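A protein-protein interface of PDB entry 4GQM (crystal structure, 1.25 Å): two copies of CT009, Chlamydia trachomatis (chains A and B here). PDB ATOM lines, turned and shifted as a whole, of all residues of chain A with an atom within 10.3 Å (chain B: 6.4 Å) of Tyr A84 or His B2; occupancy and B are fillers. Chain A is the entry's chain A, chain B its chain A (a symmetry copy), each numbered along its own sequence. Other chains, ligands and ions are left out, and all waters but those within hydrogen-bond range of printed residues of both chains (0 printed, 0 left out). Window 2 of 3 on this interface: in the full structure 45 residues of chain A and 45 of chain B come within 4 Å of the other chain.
The backbone NH (N) of Tyr A84 lies within hydrogen-bond range of the side-chain carboxylate (OE1) of Glu B10 (3.0 Å). The backbone NH (N) of Val A85 is in hydrogen-bond range of the side-chain carboxylate (OE1) of Glu B10 (2.8 Å). The backbone carbonyl oxygen of His A82 lies close to the side-chain carboxylate of Glu B10 (3.2 Å). The side-chain carboxylate (OE2) of Glu B10 sits close to the backbone nitrogen (N) of Pro A83, 3.3 Å away.
ND1 of His A82 is in hydrogen-bond range of O of Leu A78. NE2 of His B6 sits at hydrogen-bond distance from NE2 of His B2 (2.8 Å).
Among the printed residues, merely in contact across the chains: Tyr A84 with His B6 (3.6 Å), Tyr A84 with Val B7 (3.8 Å), Ile A88 with Val B7 (3.9 Å) and Tyr A84 with His B2 (3.97 Å).
Printed residues of chain B within 4 Å of Tyr A84: His B2, His B6, Val B7 and Glu B10. Printed residues of chain A within 4 Å of His B2: Tyr A84. No residue of chain A comes within 4 Å of Glu B5. Of the printed residues of chain B, His A82 touches Glu B10 (3.1 Å). Of the printed residues of chain B, Val A85 touches Glu B10. Printed residues of chain B within 4 Å of Ile A88: Val B7. Of the printed residues of chain A, Glu B10 touches His A82, Pro A83, Tyr A84 and Val A85. The nearest printed residue of chain B that does not touch His A82 is Val B7 (7.2 Å).
Hydrophobic or aromatic side chains of chain B within 4 Å of the printed part of chain A: His B2, His B6 and Val B7. Of the 16 printed residues of chain A, 5 touch a printed residue of chain B.
No position is printed for both chains. Of the 8 pairs that touch across the chains among the printed residues, none has its exchanged pair printed and touching as well.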
ATOM      1  N   MET A  64      33.712   2.963  -2.695  1.00  0.00           N
ATOM      2  CA  MET A  64      33.226   1.909  -1.816  1.00  0.00           C
ATOM      3  C   MET A  64      33.475   0.514  -2.399  1.00  0.00           C
ATOM      4  O   MET A  64      33.885  -0.404  -1.682  1.00  0.00           O
ATOM      5  CB  MET A  64      31.755   2.098  -1.499  1.00  0.00           C
ATOM      6  CG  MET A  64      31.513   3.261  -0.560  1.00  0.00           C
ATOM      7  SD  MET A  64      29.742   3.411  -0.255  1.00  0.00           S
ATOM      8  CE  MET A  64      29.724   4.731   0.957  1.00  0.00           C
ATOM      9  N   LEU A  78      27.318  -5.972  -0.462  1.00  0.00           N
ATOM     10  CA  LEU A  78      27.351  -5.056   0.663  1.00  0.00           C
ATOM     11  C   LEU A  78      26.430  -3.854   0.396  1.00  0.00           C
ATOM     12  O   LEU A  78      25.644  -3.442   1.276  1.00  0.00           O
ATOM     13  CB  LEU A  78      28.804  -4.645   0.947  1.00  0.00           C
ATOM     14  CG  LEU A  78      29.028  -3.652   2.073  1.00  0.00           C
ATOM     15  CD1 LEU A  78      28.522  -4.210   3.378  1.00  0.00           C
ATOM     16  CD2 LEU A  78      30.497  -3.306   2.176  1.00  0.00           C
ATOM     17  N   LEU A  79      26.512  -3.277  -0.800  1.00  0.00           N
ATOM     18  CA  LEU A  79      25.681  -2.124  -1.080  1.00  0.00           C
ATOM     19  C   LEU A  79      24.218  -2.538  -1.206  1.00  0.00           C
ATOM     20  O   LEU A  79      23.344  -1.798  -0.779  1.00  0.00           O
ATOM     21  CB  LEU A  79      26.215  -1.343  -2.303  1.00  0.00           C
ATOM     22  CG  LEU A  79      27.581  -0.654  -2.064  1.00  0.00           C
ATOM     23  CD1 LEU A  79      28.003   0.190  -3.246  1.00  0.00           C
ATOM     24  CD2 LEU A  79      27.635   0.138  -0.734  1.00  0.00           C
ATOM     25  N   LYS A  80      23.934  -3.732  -1.733  1.00  0.00           N
ATOM     26  CA  LYS A  80      22.557  -4.226  -1.771  1.00  0.00           C
ATOM     27  C   LYS A  80      21.938  -4.392  -0.375  1.00  0.00           C
ATOM     28  O   LYS A  80      20.719  -4.292  -0.217  1.00  0.00           O
ATOM     29  CB  LYS A  80      22.442  -5.510  -2.587  1.00  0.00           C
ATOM     30  CG  LYS A  80      22.581  -5.226  -4.084  1.00  0.00           C
ATOM     31  CD  LYS A  80      22.769  -6.510  -4.871  1.00  0.00           C
ATOM     32  CE  LYS A  80      22.827  -6.257  -6.372  1.00  0.00           C
ATOM     33  NZ  LYS A  80      23.347  -7.469  -7.115  1.00  0.00           N
ATOM     34  N   GLU A  81      22.763  -4.637   0.634  1.00  0.00           N
ATOM     35  CA  GLU A  81      22.291  -4.704   2.015  1.00  0.00           C
ATOM     36  C   GLU A  81      22.031  -3.321   2.621  1.00  0.00           C
ATOM     37  O   GLU A  81      21.598  -3.217   3.781  1.00  0.00           O
ATOM     38  CB  GLU A  81      23.314  -5.451   2.870  1.00  0.00           C
ATOM     39  CG  GLU A  81      23.414  -6.919   2.520  1.00  0.00           C
ATOM     40  CD  GLU A  81      24.596  -7.613   3.165  1.00  0.00           C
ATOM     41  OE1 GLU A  81      25.393  -6.959   3.874  1.00  0.00           O
ATOM     42  OE2 GLU A  81      24.735  -8.835   2.952  1.00  0.00           O
ATOM     43  N   HIS A  82      22.340  -2.274   1.852  1.00  0.00           N
ATOM     44  CA  HIS A  82      22.104  -0.896   2.252  1.00  0.00           C
ATOM     45  C   HIS A  82      21.255  -0.267   1.156  1.00  0.00           C
ATOM     46  O   HIS A  82      21.740   0.557   0.380  1.00  0.00           O
ATOM     47  CB  HIS A  82      23.437  -0.167   2.487  1.00  0.00           C
ATOM     48  CG  HIS A  82      24.211  -0.756   3.627  1.00  0.00           C
ATOM     49  ND1 HIS A  82      24.972  -1.898   3.505  1.00  0.00           N
ATOM     50  CD2 HIS A  82      24.244  -0.417   4.933  1.00  0.00           C
ATOM     51  CE1 HIS A  82      25.480  -2.211   4.681  1.00  0.00           C
ATOM     52  NE2 HIS A  82      25.042  -1.337   5.563  1.00  0.00           N
ATOM     53  N   PRO A  83      19.964  -0.659   1.073  1.00  0.00           N
ATOM     54  CA  PRO A  83      19.166  -0.223  -0.084  1.00  0.00           C
ATOM     55  C   PRO A  83      18.919   1.268  -0.164  1.00  0.00           C
ATOM     56  O   PRO A  83      18.733   1.786  -1.280  1.00  0.00           O
ATOM     57  CB  PRO A  83      17.840  -0.967   0.101  1.00  0.00           C
ATOM     58  CG  PRO A  83      17.807  -1.314   1.573  1.00  0.00           C
ATOM     59  CD  PRO A  83      19.236  -1.640   1.899  1.00  0.00           C
ATOM     60  N   TYR A  84      18.906   1.980   0.944  1.00  0.00           N
ATOM     61  CA  TYR A  84      18.755   3.430   0.875  1.00  0.00           C
ATOM     62  C   TYR A  84      19.996   4.092   0.268  1.00  0.00           C
ATOM     63  O   TYR A  84      19.848   5.036  -0.520  1.00  0.00           O
ATOM     64  CB  TYR A  84      18.418   4.072   2.210  1.00  0.00           C
ATOM     65  CG  TYR A  84      16.983   3.740   2.686  1.00  0.00           C
ATOM     66  CD1 TYR A  84      16.677   2.533   3.357  1.00  0.00           C
ATOM     67  CD2 TYR A  84      15.952   4.615   2.455  1.00  0.00           C
ATOM     68  CE1 TYR A  84      15.370   2.256   3.790  1.00  0.00           C
ATOM     69  CE2 TYR A  84      14.662   4.323   2.879  1.00  0.00           C
ATOM     70  CZ  TYR A  84      14.388   3.136   3.521  1.00  0.00           C
ATOM     71  OH  TYR A  84      13.089   2.878   3.949  1.00  0.00           O
ATOM     72  N   VAL A  85      21.171   3.621   0.639  1.00  0.00           N
ATOM     73  CA  VAL A  85      22.406   4.148   0.041  1.00  0.00           C
ATOM     74  C   VAL A  85      22.376   3.826  -1.430  1.00  0.00           C
ATOM     75  O   VAL A  85      22.717   4.721  -2.242  1.00  0.00           O
ATOM     76  CB  VAL A  85      23.626   3.531   0.715  1.00  0.00           C
ATOM     77  CG1 VAL A  85      24.936   3.914  -0.023  1.00  0.00           C
ATOM     78  CG2 VAL A  85      23.740   3.972   2.157  1.00  0.00           C
ATOM     79  N   LEU A  86      22.094   2.540  -1.805  1.00  0.00           N
ATOM     80  CA  LEU A  86      22.029   1.956  -3.215  1.00  0.00           C
ATOM     81  C   LEU A  86      21.098   2.720  -4.144  1.00  0.00           C
ATOM     82  O   LEU A  86      21.485   3.110  -5.247  1.00  0.00           O
ATOM     83  CB  LEU A  86      21.627   0.457  -3.215  1.00  0.00           C
ATOM     84  CG  LEU A  86      21.719  -0.339  -4.518  1.00  0.00           C
ATOM     85  CD1 LEU A  86      22.958   0.038  -5.279  1.00  0.00           C
ATOM     86  CD2 LEU A  86      21.681  -1.846  -4.223  1.00  0.00           C
ATOM     87  N   LYS A  87      19.893   2.972  -3.646  1.00  0.00           N
ATOM     88  CA  LYS A  87      18.937   3.823  -4.333  1.00  0.00           C
ATOM     89  C   LYS A  87      19.453   5.241  -4.520  1.00  0.00           C
ATOM     90  O   LYS A  87      19.330   5.802  -5.614  1.00  0.00           O
ATOM     91  CB  LYS A  87      17.602   3.823  -3.580  1.00  0.00           C
ATOM     92  CG  LYS A  87      16.572   4.809  -4.153  1.00  0.00           C
ATOM     93  CD  LYS A  87      15.769   5.471  -3.032  1.00  0.00           C
ATOM     94  N   ILE A  88      20.041   5.847  -3.500  1.00  0.00           N
ATOM     95  CA  ILE A  88      20.516   7.209  -3.728  1.00  0.00           C
ATOM     96  C   ILE A  88      21.677   7.256  -4.708  1.00  0.00           C
ATOM     97  O   ILE A  88      21.783   8.220  -5.449  1.00  0.00           O
ATOM     98  CB  ILE A  88      20.849   7.989  -2.443  1.00  0.00           C
ATOM     99  CG1 ILE A  88      22.056   7.386  -1.745  1.00  0.00           C
ATOM    100  CG2 ILE A  88      19.624   8.126  -1.560  1.00  0.00           C
ATOM    101  CD1 ILE A  88      22.743   8.369  -0.853  1.00  0.00           C
ATOM    102  N   PHE A  89      22.541   6.247  -4.726  1.00  0.00           N
ATOM    103  CA  PHE A  89      23.616   6.243  -5.735  1.00  0.00           C
ATOM    104  C   PHE A  89      23.015   6.133  -7.126  1.00  0.00           C
ATOM    105  O   PHE A  89      23.503   6.765  -8.051  1.00  0.00           O
ATOM    106  CB  PHE A  89      24.595   5.083  -5.507  1.00  0.00           C
ATOM    107  CG  PHE A  89      25.558   5.274  -4.364  1.00  0.00           C
ATOM    108  CD1 PHE A  89      25.768   6.499  -3.767  1.00  0.00           C
ATOM    109  CD2 PHE A  89      26.287   4.185  -3.902  1.00  0.00           C
ATOM    110  CE1 PHE A  89      26.690   6.647  -2.747  1.00  0.00           C
ATOM    111  CE2 PHE A  89      27.192   4.333  -2.872  1.00  0.00           C
ATOM    112  CZ  PHE A  89      27.391   5.570  -2.305  1.00  0.00           C
ATOM    113  N   GLN A  90      22.001   5.301  -7.301  1.00  0.00           N
ATOM    114  CA  GLN A  90      21.280   5.236  -8.567  1.00  0.00           C
ATOM    115  C   GLN A  90      20.664   6.583  -8.946  1.00  0.00           C
ATOM    116  O   GLN A  90      20.744   7.010 -10.097  1.00  0.00           O
ATOM    117  CB  GLN A  90      20.174   4.188  -8.489  1.00  0.00           C
ATOM    118  CG  GLN A  90      20.657   2.755  -8.366  1.00  0.00           C
ATOM    119  CD  GLN A  90      19.501   1.807  -8.166  1.00  0.00           C
ATOM    120  OE1 GLN A  90      18.481   2.177  -7.571  1.00  0.00           O
ATOM    121  NE2 GLN A  90      19.642   0.579  -8.652  1.00  0.00           N
ATOM    122  N   GLU A  91      20.088   7.266  -7.977  1.00  0.00           N
ATOM    123  CA  GLU A  91      19.478   8.563  -8.225  1.00  0.00           C
ATOM    124  C   GLU A  91      20.502   9.625  -8.591  1.00  0.00           C
ATOM    125  O   GLU A  91      20.263  10.429  -9.490  1.00  0.00           O
ATOM    126  CB  GLU A  91      18.670   9.017  -7.017  1.00  0.00           C
ATOM    127  CG  GLU A  91      17.401   8.214  -6.796  1.00  0.00           C
ATOM    128  CD  GLU A  91      16.570   8.680  -5.588  1.00  0.00           C
ATOM    129  OE1 GLU A  91      16.920   9.699  -4.943  1.00  0.00           O
ATOM    130  OE2 GLU A  91      15.552   8.023  -5.290  1.00  0.00           O
ATOM    131  N   PHE A  92      21.640   9.647  -7.908  1.00  0.00           N
ATOM    132  CA  PHE A  92      22.695  10.574  -8.284  1.00  0.00           C
ATOM    133  C   PHE A  92      23.221  10.256  -9.684  1.00  0.00           C
ATOM    134  O   PHE A  92      23.522  11.178 -10.443  1.00  0.00           O
ATOM    135  CB  PHE A  92      23.808  10.604  -7.225  1.00  0.00           C
ATOM    136  CG  PHE A  92      23.509  11.540  -6.072  1.00  0.00           C
ATOM    137  CD1 PHE A  92      23.565  12.909  -6.253  1.00  0.00           C
ATOM    138  CD2 PHE A  92      23.204  11.049  -4.809  1.00  0.00           C
ATOM    139  CE1 PHE A  92      23.304  13.756  -5.215  1.00  0.00           C
ATOM    140  CE2 PHE A  92      22.940  11.912  -3.771  1.00  0.00           C
ATOM    141  CZ  PHE A  92      22.994  13.252  -3.972  1.00  0.00           C
ATOM    142  N   GLY B   1      14.164  14.128   6.746  1.00  0.00           N
ATOM    143  CA  GLY B   1      12.896  13.374   6.971  1.00  0.00           C
ATOM    144  C   GLY B   1      13.170  11.885   7.037  1.00  0.00           C
ATOM    145  O   GLY B   1      14.301  11.480   7.294  1.00  0.00           O
ATOM    146  N   HIS B   2      12.147  11.070   6.790  1.00  0.00           N
ATOM    147  CA  HIS B   2      12.245   9.614   6.915  1.00  0.00           C
ATOM    148  C   HIS B   2      13.349   9.048   6.028  1.00  0.00           C
ATOM    149  O   HIS B   2      14.180   8.282   6.494  1.00  0.00           O
ATOM    150  CB  HIS B   2      10.883   8.979   6.579  1.00  0.00           C
ATOM    151  CG  HIS B   2      10.846   7.481   6.647  1.00  0.00           C
ATOM    152  ND1 HIS B   2      10.781   6.688   5.517  1.00  0.00           N
ATOM    153  CD2 HIS B   2      10.817   6.630   7.701  1.00  0.00           C
ATOM    154  CE1 HIS B   2      10.718   5.415   5.876  1.00  0.00           C
ATOM    155  NE2 HIS B   2      10.739   5.351   7.197  1.00  0.00           N
ATOM    156  N   MET B   3      13.360   9.428   4.755  1.00  0.00           N
ATOM    157  CA  MET B   3      14.331   8.870   3.830  1.00  0.00           C
ATOM    158  C   MET B   3      15.760   9.237   4.232  1.00  0.00           C
ATOM    159  O   MET B   3      16.661   8.366   4.275  1.00  0.00           O
ATOM    160  CB  MET B   3      14.052   9.340   2.411  1.00  0.00           C
ATOM    161  CG  MET B   3      15.084   8.841   1.418  1.00  0.00           C
ATOM    162  SD  MET B   3      14.817   9.465  -0.245  1.00  0.00           S
ATOM    163  CE  MET B   3      13.202   8.795  -0.634  1.00  0.00           C
ATOM    164  N   SER B   4      15.974  10.518   4.545  1.00  0.00           N
ATOM    165  CA  SER B   4      17.325  10.911   4.932  1.00  0.00           C
ATOM    166  C   SER B   4      17.762  10.234   6.228  1.00  0.00           C
ATOM    167  O   SER B   4      18.922   9.868   6.390  1.00  0.00           O
ATOM    168  CB  SER B   4      17.494  12.431   5.001  1.00  0.00           C
ATOM    169  OG  SER B   4      16.709  12.980   6.024  1.00  0.00           O
ATOM    170  N   GLU B   5      16.837  10.044   7.148  1.00  0.00           N
ATOM    171  CA  GLU B   5      17.213   9.362   8.378  1.00  0.00           C
ATOM    172  C   GLU B   5      17.665   7.914   8.114  1.00  0.00           C
ATOM    173  O   GLU B   5      18.673   7.477   8.687  1.00  0.00           O
ATOM    174  CB  GLU B   5      16.080   9.465   9.399  1.00  0.00           C
ATOM    175  CG  GLU B   5      15.983  10.918   9.941  1.00  0.00           C
ATOM    176  CD  GLU B   5      14.637  11.272  10.512  1.00  0.00           C
ATOM    177  OE1 GLU B   5      13.857  10.344  10.760  1.00  0.00           O
ATOM    178  OE2 GLU B   5      14.341  12.465  10.718  1.00  0.00           O
ATOM    179  N   HIS B   6      16.982   7.202   7.206  1.00  0.00           N
ATOM    180  CA  HIS B   6      17.453   5.846   6.870  1.00  0.00           C
ATOM    181  C   HIS B   6      18.824   5.885   6.165  1.00  0.00           C
ATOM    182  O   HIS B   6      19.671   5.071   6.443  1.00  0.00           O
ATOM    183  CB  HIS B   6      16.479   5.113   5.957  1.00  0.00           C
ATOM    184  CG  HIS B   6      15.263   4.585   6.648  1.00  0.00           C
ATOM    185  ND1 HIS B   6      15.280   3.426   7.387  1.00  0.00           N
ATOM    186  CD2 HIS B   6      14.002   5.050   6.683  1.00  0.00           C
ATOM    187  CE1 HIS B   6      14.068   3.189   7.845  1.00  0.00           C
ATOM    188  NE2 HIS B   6      13.269   4.150   7.431  1.00  0.00           N
ATOM    189  N   VAL B   7      19.024   6.824   5.238  1.00  0.00           N
ATOM    190  CA  VAL B   7      20.284   6.962   4.501  1.00  0.00           C
ATOM    191  C   VAL B   7      21.453   7.163   5.469  1.00  0.00           C
ATOM    192  O   VAL B   7      22.458   6.507   5.394  1.00  0.00           O
ATOM    193  CB  VAL B   7      20.225   8.160   3.495  1.00  0.00           C
ATOM    194  CG1 VAL B   7      21.625   8.558   2.972  1.00  0.00           C
ATOM    195  CG2 VAL B   7      19.278   7.813   2.330  1.00  0.00           C
ATOM    196  N   GLU B  10      22.138   4.026   7.565  1.00  0.00           N
ATOM    197  CA  GLU B  10      22.827   3.031   6.756  1.00  0.00           C
ATOM    198  C   GLU B  10      24.277   3.427   6.520  1.00  0.00           C
ATOM    199  O   GLU B  10      25.161   2.572   6.566  1.00  0.00           O
ATOM    200  CB  GLU B  10      22.191   2.826   5.399  1.00  0.00           C
ATOM    201  CG  GLU B  10      20.913   1.961   5.426  1.00  0.00           C
ATOM    202  CD  GLU B  10      20.435   1.615   4.050  1.00  0.00           C
ATOM    203  OE1 GLU B  10      21.009   2.129   3.046  1.00  0.00           O
ATOM    204  OE2 GLU B  10      19.451   0.841   3.952  1.00  0.00           O
ATOM    205  N   GLU B 104      17.225  16.171   2.828  1.00  0.00           N
ATOM    206  CA  GLU B 104      16.781  16.379   4.207  1.00  0.00           C
ATOM    207  C   GLU B 104      15.286  16.720   4.277  1.00  0.00           C
ATOM    208  O   GLU B 104      14.581  16.307   5.198  1.00  0.00           O
ATOM    209  CB  GLU B 104      17.610  17.481   4.866  1.00  0.00           C
ATOM    210  CG  GLU B 104      19.072  17.123   5.005  1.00  0.00           C
ATOM    211  CD  GLU B 104      19.264  15.791   5.699  1.00  0.00           C
ATOM    212  OE1 GLU B 104      18.674  15.594   6.789  1.00  0.00           O
ATOM    213  OE2 GLU B 104      19.988  14.935   5.146  1.00  0.00           O
